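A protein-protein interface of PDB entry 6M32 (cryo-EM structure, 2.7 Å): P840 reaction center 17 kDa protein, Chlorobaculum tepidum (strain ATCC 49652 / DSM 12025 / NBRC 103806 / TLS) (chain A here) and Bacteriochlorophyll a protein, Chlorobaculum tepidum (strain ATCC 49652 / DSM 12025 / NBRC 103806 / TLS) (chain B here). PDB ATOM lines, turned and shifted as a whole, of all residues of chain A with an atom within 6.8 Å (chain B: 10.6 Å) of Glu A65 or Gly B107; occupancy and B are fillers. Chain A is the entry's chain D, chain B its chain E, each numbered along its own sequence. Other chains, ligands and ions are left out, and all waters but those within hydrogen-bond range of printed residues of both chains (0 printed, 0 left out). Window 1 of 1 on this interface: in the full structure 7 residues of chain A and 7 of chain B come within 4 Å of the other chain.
The guanidinium group (NH2) of Arg A58 lies within hydrogen-bond range of the side-chain hydroxyl (OG) of Ser B77, at 3.2 Å. OG1 of Thr B78 sits at hydrogen-bond distance from NH2 of Arg A58 (3.3 Å). The guanidinium group (NH2) of Arg A69 is in hydrogen-bond range of the backbone carbonyl oxygen (O) of Gly B107 (2.9 Å). OE1 of Glu A65 sits close to O of Gly B107, 3.1 Å away. The side-chain carboxylate (OE1) of Glu A65 sits close to the backbone carbonyl oxygen (O) of Asp B108 (3.0 Å).
OG of Ser B77 sits close to OD1 of Asp B76, at 3.5 Å. OG1 of Thr B78 sits at hydrogen-bond distance from O of Asp B76, 3.3 Å away. O of Lys B79 is in hydrogen-bond range of N of Gly B107 (3.0 Å). The backbone NH of Lys B81 lies within hydrogen-bond range of the backbone carbonyl oxygen of Ser B105 (2.9 Å). The guanidinium group of Arg A68 is in salt-bridge range of the side-chain carboxylate of Glu A65 (2.6 Å). NH2 of Arg A69 is in salt-bridge range of OE2 of Glu A65, at 3.1 Å.
CD2 of Leu A60 touches OD1 of Asp B108, at 3.0 Å. Thr A63 touches Asp B108 (CG2 to O, 3.1 Å). CB of Glu A65 touches OG of Ser B110, 3.3 Å away. Met A66 touches Asp B108 (CG to CB, 3.4 Å). Arg A68 touches Ser B105 (NH2 to OG, 3.99 Å). Arg A69 touches Lys B79 (NH1 to CD, 3.8 Å).
Of the printed residues of chain B, Leu A60 touches Asp B108. No residue of chain B comes within 4 Å of Pro A64. Of chain B, only Asp B108 comes within 4 Å of Met A66. No residue of chain B comes within 4 Å of Ile A67. Printed residues of chain A within 4 Å of Thr B78: Arg A58. Of the printed residues of chain A, Lys B79 touches Arg A69 (3.8 Å). Of the printed residues of chain A, Ser B105 touches Arg A68. Of chain A, only Glu A65 (3.1 Å) and Arg A69 (2.9 Å) come within 4 Å of Gly B107. Of the printed residues of chain A, Asp B108 touches Leu A60 (3.0 Å), Thr A63 (3.1 Å), Glu A65 (3.0 Å) and Met A66 (3.4 Å). Phe B109 touches none of the printed residues of chain A. The nearest residue of chain A that does not touch Gly B107 is Met A66 (4.3 Å). The nearest printed residue of chain A that does not touch Ser B105 is Glu A65 (4.5 Å).
Printed residues of chain B that touch a printed residue of chain A: Ser B77, Thr B78, Lys B79, Ser B105, Gly B107, Asp B108 and Ser B110. Along chain B the printed residues that touch a printed residue of chain A span positions 77 to 110. Of the 11 printed residues of chain A, 7 touch a printed residue of chain B. Hydrophobic or aromatic side chains of chain A within 4 Å of the printed part of chain B: Leu A60 and Met A66. Along chain A the printed residues that touch a printed residue of chain B span positions 58 to 69.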
ATOM      1  N   ARG A  58      32.194   1.284 -16.296  1.00  0.00           N
ATOM      2  CA  ARG A  58      31.910  -0.124 -16.512  1.00  0.00           C
ATOM      3  C   ARG A  58      31.043  -0.268 -17.754  1.00  0.00           C
ATOM      4  O   ARG A  58      30.480   0.704 -18.261  1.00  0.00           O
ATOM      5  CB  ARG A  58      31.206  -0.748 -15.302  1.00  0.00           C
ATOM      6  CG  ARG A  58      31.924  -0.585 -13.979  1.00  0.00           C
ATOM      7  CD  ARG A  58      30.929  -0.429 -12.844  1.00  0.00           C
ATOM      8  NE  ARG A  58      31.578  -0.467 -11.539  1.00  0.00           N
ATOM      9  CZ  ARG A  58      32.191   0.570 -10.982  1.00  0.00           C
ATOM     10  NH1 ARG A  58      32.237   1.733 -11.615  1.00  0.00           N
ATOM     11  NH2 ARG A  58      32.755   0.448  -9.789  1.00  0.00           N
ATOM     12  N   LEU A  60      28.191  -3.076 -18.522  1.00  0.00           N
ATOM     13  CA  LEU A  60      27.509  -4.237 -17.976  1.00  0.00           C
ATOM     14  C   LEU A  60      26.514  -4.801 -18.993  1.00  0.00           C
ATOM     15  O   LEU A  60      26.492  -4.405 -20.160  1.00  0.00           O
ATOM     16  CB  LEU A  60      26.832  -3.873 -16.657  1.00  0.00           C
ATOM     17  CG  LEU A  60      27.621  -2.977 -15.700  1.00  0.00           C
ATOM     18  CD1 LEU A  60      26.930  -2.918 -14.356  1.00  0.00           C
ATOM     19  CD2 LEU A  60      29.053  -3.448 -15.539  1.00  0.00           C
ATOM     20  N   PRO A  62      22.375  -7.225 -19.355  1.00  0.00           N
ATOM     21  CA  PRO A  62      21.118  -7.562 -18.680  1.00  0.00           C
ATOM     22  C   PRO A  62      21.316  -8.293 -17.366  1.00  0.00           C
ATOM     23  O   PRO A  62      20.891  -7.800 -16.318  1.00  0.00           O
ATOM     24  CB  PRO A  62      20.434  -8.474 -19.703  1.00  0.00           C
ATOM     25  CG  PRO A  62      20.973  -7.989 -21.058  1.00  0.00           C
ATOM     26  CD  PRO A  62      22.098  -7.004 -20.781  1.00  0.00           C
ATOM     27  N   THR A  63      21.962  -9.465 -17.422  1.00  0.00           N
ATOM     28  CA  THR A  63      22.519 -10.117 -16.243  1.00  0.00           C
ATOM     29  C   THR A  63      21.483 -10.250 -15.131  1.00  0.00           C
ATOM     30  O   THR A  63      21.459  -9.418 -14.218  1.00  0.00           O
ATOM     31  CB  THR A  63      23.745  -9.358 -15.744  1.00  0.00           C
ATOM     32  OG1 THR A  63      24.619  -9.095 -16.848  1.00  0.00           O
ATOM     33  CG2 THR A  63      24.496 -10.204 -14.741  1.00  0.00           C
ATOM     34  N   PRO A  64      20.608 -11.270 -15.184  1.00  0.00           N
ATOM     35  CA  PRO A  64      19.392 -11.295 -14.350  1.00  0.00           C
ATOM     36  C   PRO A  64      19.549 -10.822 -12.909  1.00  0.00           C
ATOM     37  O   PRO A  64      18.556 -10.468 -12.270  1.00  0.00           O
ATOM     38  CB  PRO A  64      18.987 -12.774 -14.386  1.00  0.00           C
ATOM     39  CG  PRO A  64      19.543 -13.288 -15.664  1.00  0.00           C
ATOM     40  CD  PRO A  64      20.798 -12.521 -15.938  1.00  0.00           C
ATOM     41  N   GLU A  65      20.770 -10.835 -12.373  1.00  0.00           N
ATOM     42  CA  GLU A  65      21.022 -10.147 -11.110  1.00  0.00           C
ATOM     43  C   GLU A  65      20.775  -8.645 -11.238  1.00  0.00           C
ATOM     44  O   GLU A  65      20.152  -8.029 -10.359  1.00  0.00           O
ATOM     45  CB  GLU A  65      22.449 -10.439 -10.650  1.00  0.00           C
ATOM     46  CG  GLU A  65      22.777 -10.002  -9.237  1.00  0.00           C
ATOM     47  CD  GLU A  65      23.164  -8.546  -9.164  1.00  0.00           C
ATOM     48  OE1 GLU A  65      23.685  -8.027 -10.171  1.00  0.00           O
ATOM     49  OE2 GLU A  65      22.961  -7.920  -8.105  1.00  0.00           O
ATOM     50  N   MET A  66      21.250  -8.032 -12.325  1.00  0.00           N
ATOM     51  CA  MET A  66      20.910  -6.635 -12.572  1.00  0.00           C
ATOM     52  C   MET A  66      19.408  -6.458 -12.713  1.00  0.00           C
ATOM     53  O   MET A  66      18.852  -5.459 -12.254  1.00  0.00           O
ATOM     54  CB  MET A  66      21.621  -6.113 -13.817  1.00  0.00           C
ATOM     55  CG  MET A  66      23.118  -6.049 -13.687  1.00  0.00           C
ATOM     56  SD  MET A  66      23.651  -4.946 -12.364  1.00  0.00           S
ATOM     57  CE  MET A  66      23.196  -3.357 -13.043  1.00  0.00           C
ATOM     58  N   ILE A  67      18.732  -7.421 -13.340  1.00  0.00           N
ATOM     59  CA  ILE A  67      17.286  -7.321 -13.501  1.00  0.00           C
ATOM     60  C   ILE A  67      16.573  -7.387 -12.157  1.00  0.00           C
ATOM     61  O   ILE A  67      15.618  -6.635 -11.918  1.00  0.00           O
ATOM     62  CB  ILE A  67      16.791  -8.411 -14.468  1.00  0.00           C
ATOM     63  CG1 ILE A  67      17.294  -8.114 -15.881  1.00  0.00           C
ATOM     64  CG2 ILE A  67      15.277  -8.498 -14.440  1.00  0.00           C
ATOM     65  CD1 ILE A  67      17.103  -9.251 -16.852  1.00  0.00           C
ATOM     66  N   ARG A  68      17.009  -8.272 -11.256  1.00  0.00           N
ATOM     67  CA  ARG A  68      16.337  -8.371  -9.964  1.00  0.00           C
ATOM     68  C   ARG A  68      16.590  -7.128  -9.124  1.00  0.00           C
ATOM     69  O   ARG A  68      15.705  -6.679  -8.387  1.00  0.00           O
ATOM     70  CB  ARG A  68      16.762  -9.636  -9.205  1.00  0.00           C
ATOM     71  CG  ARG A  68      18.245  -9.769  -8.902  1.00  0.00           C
ATOM     72  CD  ARG A  68      18.647  -9.099  -7.592  1.00  0.00           C
ATOM     73  NE  ARG A  68      20.041  -9.356  -7.238  1.00  0.00           N
ATOM     74  CZ  ARG A  68      20.671  -8.779  -6.219  1.00  0.00           C
ATOM     75  NH1 ARG A  68      20.039  -7.892  -5.462  1.00  0.00           N
ATOM     76  NH2 ARG A  68      21.941  -9.071  -5.969  1.00  0.00           N
ATOM     77  N   ARG A  69      17.791  -6.551  -9.215  1.00  0.00           N
ATOM     78  CA  ARG A  69      17.969  -5.309  -8.472  1.00  0.00           C
ATOM     79  C   ARG A  69      17.300  -4.130  -9.162  1.00  0.00           C
ATOM     80  O   ARG A  69      17.048  -3.110  -8.513  1.00  0.00           O
ATOM     81  CB  ARG A  69      19.447  -5.005  -8.232  1.00  0.00           C
ATOM     82  CG  ARG A  69      20.269  -4.685  -9.460  1.00  0.00           C
ATOM     83  CD  ARG A  69      21.532  -3.964  -9.028  1.00  0.00           C
ATOM     84  NE  ARG A  69      22.481  -4.869  -8.391  1.00  0.00           N
ATOM     85  CZ  ARG A  69      23.627  -4.483  -7.842  1.00  0.00           C
ATOM     86  NH1 ARG A  69      23.965  -3.201  -7.848  1.00  0.00           N
ATOM     87  NH2 ARG A  69      24.432  -5.375  -7.281  1.00  0.00           N
ATOM     88  N   LEU A  70      17.016  -4.247 -10.458  1.00  0.00           N
ATOM     89  CA  LEU A  70      16.199  -3.255 -11.142  1.00  0.00           C
ATOM     90  C   LEU A  70      14.776  -3.269 -10.611  1.00  0.00           C
ATOM     91  O   LEU A  70      14.234  -2.229 -10.218  1.00  0.00           O
ATOM     92  CB  LEU A  70      16.183  -3.553 -12.640  1.00  0.00           C
ATOM     93  CG  LEU A  70      15.538  -2.539 -13.578  1.00  0.00           C
ATOM     94  CD1 LEU A  70      16.160  -2.680 -14.926  1.00  0.00           C
ATOM     95  CD2 LEU A  70      14.070  -2.701 -13.684  1.00  0.00           C
ATOM     96  N   PHE B  71      26.632 -10.842   4.143  1.00  0.00           N
ATOM     97  CA  PHE B  71      27.644  -9.802   4.042  1.00  0.00           C
ATOM     98  C   PHE B  71      27.306  -8.881   2.882  1.00  0.00           C
ATOM     99  O   PHE B  71      27.121  -9.346   1.755  1.00  0.00           O
ATOM    100  CB  PHE B  71      29.038 -10.392   3.811  1.00  0.00           C
ATOM    101  CG  PHE B  71      29.498 -11.336   4.882  1.00  0.00           C
ATOM    102  CD1 PHE B  71      30.286 -10.882   5.921  1.00  0.00           C
ATOM    103  CD2 PHE B  71      29.168 -12.678   4.838  1.00  0.00           C
ATOM    104  CE1 PHE B  71      30.727 -11.743   6.902  1.00  0.00           C
ATOM    105  CE2 PHE B  71      29.604 -13.542   5.819  1.00  0.00           C
ATOM    106  CZ  PHE B  71      30.383 -13.074   6.851  1.00  0.00           C
ATOM    107  N   GLU B  72      27.235  -7.583   3.155  1.00  0.00           N
ATOM    108  CA  GLU B  72      27.247  -6.568   2.113  1.00  0.00           C
ATOM    109  C   GLU B  72      28.426  -5.642   2.335  1.00  0.00           C
ATOM    110  O   GLU B  72      28.777  -5.328   3.475  1.00  0.00           O
ATOM    111  CB  GLU B  72      25.960  -5.735   2.064  1.00  0.00           C
ATOM    112  CG  GLU B  72      24.713  -6.478   1.636  1.00  0.00           C
ATOM    113  CD  GLU B  72      24.065  -7.238   2.762  1.00  0.00           C
ATOM    114  OE1 GLU B  72      24.553  -7.142   3.906  1.00  0.00           O
ATOM    115  OE2 GLU B  72      23.047  -7.912   2.505  1.00  0.00           O
ATOM    116  N   SER B  73      29.034  -5.211   1.238  1.00  0.00           N
ATOM    117  CA  SER B  73      30.121  -4.254   1.315  1.00  0.00           C
ATOM    118  C   SER B  73      30.082  -3.377   0.079  1.00  0.00           C
ATOM    119  O   SER B  73      29.593  -3.779  -0.977  1.00  0.00           O
ATOM    120  CB  SER B  73      31.487  -4.941   1.433  1.00  0.00           C
ATOM    121  OG  SER B  73      31.803  -5.653   0.252  1.00  0.00           O
ATOM    122  N   ILE B  74      30.592  -2.162   0.227  1.00  0.00           N
ATOM    123  CA  ILE B  74      30.830  -1.269  -0.897  1.00  0.00           C
ATOM    124  C   ILE B  74      32.318  -0.969  -0.865  1.00  0.00           C
ATOM    125  O   ILE B  74      32.797  -0.249   0.017  1.00  0.00           O
ATOM    126  CB  ILE B  74      29.994   0.012  -0.831  1.00  0.00           C
ATOM    127  CG1 ILE B  74      28.520  -0.325  -1.064  1.00  0.00           C
ATOM    128  CG2 ILE B  74      30.483   1.024  -1.857  1.00  0.00           C
ATOM    129  CD1 ILE B  74      27.643   0.871  -1.330  1.00  0.00           C
ATOM    130  N   VAL B  75      33.059  -1.542  -1.807  1.00  0.00           N
ATOM    131  CA  VAL B  75      34.504  -1.382  -1.839  1.00  0.00           C
ATOM    132  C   VAL B  75      34.883  -0.545  -3.045  1.00  0.00           C
ATOM    133  O   VAL B  75      34.944  -1.056  -4.168  1.00  0.00           O
ATOM    134  CB  VAL B  75      35.226  -2.737  -1.882  1.00  0.00           C
ATOM    135  CG1 VAL B  75      36.723  -2.516  -1.847  1.00  0.00           C
ATOM    136  CG2 VAL B  75      34.788  -3.607  -0.720  1.00  0.00           C
ATOM    137  N   ASP B  76      35.149   0.739  -2.817  1.00  0.00           N
ATOM    138  CA  ASP B  76      35.515   1.638  -3.898  1.00  0.00           C
ATOM    139  C   ASP B  76      34.489   1.538  -5.018  1.00  0.00           C
ATOM    140  O   ASP B  76      34.802   1.019  -6.092  1.00  0.00           O
ATOM    141  CB  ASP B  76      36.907   1.303  -4.430  1.00  0.00           C
ATOM    142  CG  ASP B  76      37.381   2.269  -5.496  1.00  0.00           C
ATOM    143  OD1 ASP B  76      36.627   3.208  -5.800  1.00  0.00           O
ATOM    144  OD2 ASP B  76      38.491   2.094  -6.029  1.00  0.00           O
ATOM    145  N   SER B  77      33.251   1.955  -4.756  1.00  0.00           N
ATOM    146  CA  SER B  77      32.222   2.036  -5.792  1.00  0.00           C
ATOM    147  C   SER B  77      31.945   0.675  -6.432  1.00  0.00           C
ATOM    148  O   SER B  77      31.873   0.544  -7.655  1.00  0.00           O
ATOM    149  CB  SER B  77      32.613   3.066  -6.854  1.00  0.00           C
ATOM    150  OG  SER B  77      33.728   2.615  -7.609  1.00  0.00           O
ATOM    151  N   THR B  78      31.798  -0.348  -5.592  1.00  0.00           N
ATOM    152  CA  THR B  78      31.536  -1.703  -6.069  1.00  0.00           C
ATOM    153  C   THR B  78      30.780  -2.454  -4.986  1.00  0.00           C
ATOM    154  O   THR B  78      31.317  -2.654  -3.894  1.00  0.00           O
ATOM    155  CB  THR B  78      32.832  -2.444  -6.399  1.00  0.00           C
ATOM    156  OG1 THR B  78      33.573  -1.720  -7.386  1.00  0.00           O
ATOM    157  CG2 THR B  78      32.511  -3.818  -6.947  1.00  0.00           C
ATOM    158  N   LYS B  79      29.557  -2.883  -5.283  1.00  0.00           N
ATOM    159  CA  LYS B  79      28.737  -3.587  -4.305  1.00  0.00           C
ATOM    160  C   LYS B  79      29.027  -5.082  -4.331  1.00  0.00           C
ATOM    161  O   LYS B  79      28.979  -5.714  -5.390  1.00  0.00           O
ATOM    162  CB  LYS B  79      27.251  -3.342  -4.560  1.00  0.00           C
ATOM    163  CG  LYS B  79      26.800  -1.929  -4.253  1.00  0.00           C
ATOM    164  CD  LYS B  79      25.325  -1.750  -4.566  1.00  0.00           C
ATOM    165  CE  LYS B  79      24.956  -0.286  -4.734  1.00  0.00           C
ATOM    166  NZ  LYS B  79      25.943   0.617  -4.093  1.00  0.00           N
ATOM    167  N   ASN B  80      29.312  -5.641  -3.160  1.00  0.00           N
ATOM    168  CA  ASN B  80      29.587  -7.057  -2.998  1.00  0.00           C
ATOM    169  C   ASN B  80      28.636  -7.644  -1.966  1.00  0.00           C
ATOM    170  O   ASN B  80      28.379  -7.041  -0.922  1.00  0.00           O
ATOM    171  CB  ASN B  80      31.034  -7.285  -2.561  1.00  0.00           C
ATOM    172  CG  ASN B  80      32.026  -6.689  -3.526  1.00  0.00           C
ATOM    173  OD1 ASN B  80      31.754  -6.575  -4.718  1.00  0.00           O
ATOM    174  ND2 ASN B  80      33.181  -6.291  -3.015  1.00  0.00           N
ATOM    175  N   LYS B  81      28.120  -8.833  -2.264  1.00  0.00           N
ATOM    176  CA  LYS B  81      27.194  -9.498  -1.364  1.00  0.00           C
ATOM    177  C   LYS B  81      27.529 -10.980  -1.306  1.00  0.00           C
ATOM    178  O   LYS B  81      27.834 -11.595  -2.329  1.00  0.00           O
ATOM    179  CB  LYS B  81      25.741  -9.299  -1.808  1.00  0.00           C
ATOM    180  CG  LYS B  81      24.716  -9.881  -0.858  1.00  0.00           C
ATOM    181  CD  LYS B  81      23.345  -9.320  -1.152  1.00  0.00           C
ATOM    182  CE  LYS B  81      22.328  -9.805  -0.146  1.00  0.00           C
ATOM    183  NZ  LYS B  81      20.991  -9.227  -0.430  1.00  0.00           N
ATOM    184  N   LEU B  82      27.473 -11.538  -0.101  1.00  0.00           N
ATOM    185  CA  LEU B  82      27.723 -12.962   0.110  1.00  0.00           C
ATOM    186  C   LEU B  82      26.701 -13.477   1.106  1.00  0.00           C
ATOM    187  O   LEU B  82      26.657 -13.008   2.245  1.00  0.00           O
ATOM    188  CB  LEU B  82      29.134 -13.211   0.625  1.00  0.00           C
ATOM    189  CG  LEU B  82      29.525 -14.677   0.815  1.00  0.00           C
ATOM    190  CD1 LEU B  82      30.343 -15.175  -0.359  1.00  0.00           C
ATOM    191  CD2 LEU B  82      30.277 -14.864   2.123  1.00  0.00           C
ATOM    192  N   THR B  83      25.897 -14.441   0.688  1.00  0.00           N
ATOM    193  CA  THR B  83      24.943 -15.082   1.573  1.00  0.00           C
ATOM    194  C   THR B  83      25.297 -16.552   1.730  1.00  0.00           C
ATOM    195  O   THR B  83      25.629 -17.239   0.764  1.00  0.00           O
ATOM    196  CB  THR B  83      23.521 -14.921   1.033  1.00  0.00           C
ATOM    197  OG1 THR B  83      23.450 -15.505  -0.270  1.00  0.00           O
ATOM    198  CG2 THR B  83      23.099 -13.450   0.966  1.00  0.00           C
ATOM    199  N   MET B 103      25.116 -18.013  -1.960  1.00  0.00           N
ATOM    200  CA  MET B 103      25.421 -17.365  -3.229  1.00  0.00           C
ATOM    201  C   MET B 103      26.386 -16.215  -2.989  1.00  0.00           C
ATOM    202  O   MET B 103      26.538 -15.722  -1.870  1.00  0.00           O
ATOM    203  CB  MET B 103      24.153 -16.860  -3.918  1.00  0.00           C
ATOM    204  CG  MET B 103      23.468 -15.734  -3.189  1.00  0.00           C
ATOM    205  SD  MET B 103      22.063 -14.999  -4.059  1.00  0.00           S
ATOM    206  CE  MET B 103      22.903 -13.974  -5.241  1.00  0.00           C
ATOM    207  N   VAL B 104      27.040 -15.793  -4.061  1.00  0.00           N
ATOM    208  CA  VAL B 104      27.923 -14.632  -4.027  1.00  0.00           C
ATOM    209  C   VAL B 104      27.664 -13.795  -5.270  1.00  0.00           C
ATOM    210  O   VAL B 104      27.531 -14.330  -6.376  1.00  0.00           O
ATOM    211  CB  VAL B 104      29.403 -15.062  -3.905  1.00  0.00           C
ATOM    212  CG1 VAL B 104      29.756 -16.036  -5.004  1.00  0.00           C
ATOM    213  CG2 VAL B 104      30.320 -13.855  -3.966  1.00  0.00           C
ATOM    214  N   SER B 105      27.569 -12.478  -5.076  1.00  0.00           N
ATOM    215  CA  SER B 105      27.289 -11.546  -6.159  1.00  0.00           C
ATOM    216  C   SER B 105      28.238 -10.365  -6.056  1.00  0.00           C
ATOM    217  O   SER B 105      28.360  -9.751  -4.994  1.00  0.00           O
ATOM    218  CB  SER B 105      25.842 -11.049  -6.105  1.00  0.00           C
ATOM    219  OG  SER B 105      25.629 -10.219  -4.978  1.00  0.00           O
ATOM    220  N   VAL B 106      28.902 -10.045  -7.160  1.00  0.00           N
ATOM    221  CA  VAL B 106      29.778  -8.886  -7.257  1.00  0.00           C
ATOM    222  C   VAL B 106      29.328  -8.061  -8.449  1.00  0.00           C
ATOM    223  O   VAL B 106      29.241  -8.580  -9.567  1.00  0.00           O
ATOM    224  CB  VAL B 106      31.254  -9.289  -7.401  1.00  0.00           C
ATOM    225  CG1 VAL B 106      32.120  -8.054  -7.600  1.00  0.00           C
ATOM    226  CG2 VAL B 106      31.705 -10.073  -6.181  1.00  0.00           C
ATOM    227  N   GLY B 107      29.033  -6.787  -8.210  1.00  0.00           N
ATOM    228  CA  GLY B 107      28.567  -5.917  -9.268  1.00  0.00           C
ATOM    229  C   GLY B 107      27.315  -6.449  -9.931  1.00  0.00           C
ATOM    230  O   GLY B 107      26.236  -6.436  -9.336  1.00  0.00           O
ATOM    231  N   ASP B 108      27.451  -6.923 -11.170  1.00  0.00           N
ATOM    232  CA  ASP B 108      26.361  -7.587 -11.867  1.00  0.00           C
ATOM    233  C   ASP B 108      26.452  -9.103 -11.827  1.00  0.00           C
ATOM    234  O   ASP B 108      25.412  -9.769 -11.853  1.00  0.00           O
ATOM    235  CB  ASP B 108      26.313  -7.139 -13.332  1.00  0.00           C
ATOM    236  CG  ASP B 108      27.671  -7.175 -13.996  1.00  0.00           C
ATOM    237  OD1 ASP B 108      28.036  -6.182 -14.652  1.00  0.00           O
ATOM    238  OD2 ASP B 108      28.380  -8.195 -13.862  1.00  0.00           O
ATOM    239  N   PHE B 109      27.658  -9.658 -11.767  1.00  0.00           N
ATOM    240  CA  PHE B 109      27.826 -11.101 -11.753  1.00  0.00           C
ATOM    241  C   PHE B 109      27.318 -11.689 -10.445  1.00  0.00           C
ATOM    242  O   PHE B 109      27.427 -11.077  -9.382  1.00  0.00           O
ATOM    243  CB  PHE B 109      29.296 -11.459 -11.956  1.00  0.00           C
ATOM    244  CG  PHE B 109      29.589 -12.920 -11.815  1.00  0.00           C
ATOM    245  CD1 PHE B 109      29.292 -13.799 -12.837  1.00  0.00           C
ATOM    246  CD2 PHE B 109      30.167 -13.413 -10.662  1.00  0.00           C
ATOM    247  CE1 PHE B 109      29.562 -15.140 -12.707  1.00  0.00           C
ATOM    248  CE2 PHE B 109      30.438 -14.752 -10.528  1.00  0.00           C
ATOM    249  CZ  PHE B 109      30.137 -15.617 -11.551  1.00  0.00           C
ATOM    250  N   SER B 110      26.747 -12.885 -10.530  1.00  0.00           N
ATOM    251  CA  SER B 110      26.244 -13.565  -9.348  1.00  0.00           C
ATOM    252  C   SER B 110      26.130 -15.049  -9.645  1.00  0.00           C
ATOM    253  O   SER B 110      25.868 -15.445 -10.783  1.00  0.00           O
ATOM    254  CB  SER B 110      24.886 -13.006  -8.913  1.00  0.00           C
ATOM    255  OG  SER B 110      23.894 -13.262  -9.889  1.00  0.00           O
ATOM    256  N   HIS B 111      26.330 -15.865  -8.612  1.00  0.00           N
ATOM    257  CA  HIS B 111      26.104 -17.295  -8.770  1.00  0.00           C
ATOM    258  C   HIS B 111      25.882 -17.931  -7.407  1.00  0.00           C
ATOM    259  O   HIS B 111      26.402 -17.458  -6.392  1.00  0.00           O
ATOM    260  CB  HIS B 111      27.270 -17.981  -9.485  1.00  0.00           C
ATOM    261  CG  HIS B 111      28.483 -18.150  -8.631  1.00  0.00           C
ATOM    262  ND1 HIS B 111      28.748 -19.311  -7.940  1.00  0.00           N
ATOM    263  CD2 HIS B 111      29.499 -17.302  -8.347  1.00  0.00           C
ATOM    264  CE1 HIS B 111      29.877 -19.173  -7.270  1.00  0.00           C
ATOM    265  NE2 HIS B 111      30.351 -17.963  -7.500  1.00  0.00           N
ATOM    266  N   THR B 112      25.114 -19.016  -7.406  1.00  0.00           N
ATOM    267  CA  THR B 112      24.790 -19.766  -6.203  1.00  0.00           C
ATOM    268  C   THR B 112      25.668 -21.007  -6.096  1.00  0.00           C
ATOM    269  O   THR B 112      26.384 -21.375  -7.028  1.00  0.00           O
ATOM    270  CB  THR B 112      23.314 -20.171  -6.196  1.00  0.00           C
ATOM    271  OG1 THR B 112      23.067 -21.090  -7.267  1.00  0.00           O
ATOM    272  CG2 THR B 112      22.431 -18.957  -6.377  1.00  0.00           C
ATOM    273  N   ASP B 155      25.574 -21.526 -15.540  1.00  0.00           N
ATOM    274  CA  ASP B 155      24.552 -20.914 -16.379  1.00  0.00           C
ATOM    275  C   ASP B 155      25.088 -19.696 -17.120  1.00  0.00           C
ATOM    276  O   ASP B 155      24.641 -19.390 -18.229  1.00  0.00           O
ATOM    277  CB  ASP B 155      23.339 -20.537 -15.529  1.00  0.00           C
ATOM    278  CG  ASP B 155      23.715 -19.733 -14.301  1.00  0.00           C
ATOM    279  OD1 ASP B 155      24.810 -19.132 -14.289  1.00  0.00           O
ATOM    280  OD2 ASP B 155      22.921 -19.711 -13.339  1.00  0.00           O
ATOM    281  N   ASN B 156      26.036 -18.993 -16.517  1.00  0.00           N
ATOM    282  CA  ASN B 156      26.657 -17.850 -17.164  1.00  0.00           C
ATOM    283  C   ASN B 156      27.769 -18.313 -18.093  1.00  0.00           C
ATOM    284  O   ASN B 156      28.302 -19.417 -17.956  1.00  0.00           O
ATOM    285  CB  ASN B 156      27.217 -16.873 -16.131  1.00  0.00           C
ATOM    286  CG  ASN B 156      26.132 -16.121 -15.391  1.00  0.00           C
ATOM    287  OD1 ASN B 156      24.950 -16.446 -15.510  1.00  0.00           O
ATOM    288  ND2 ASN B 156      26.522 -15.105 -14.629  1.00  0.00           N
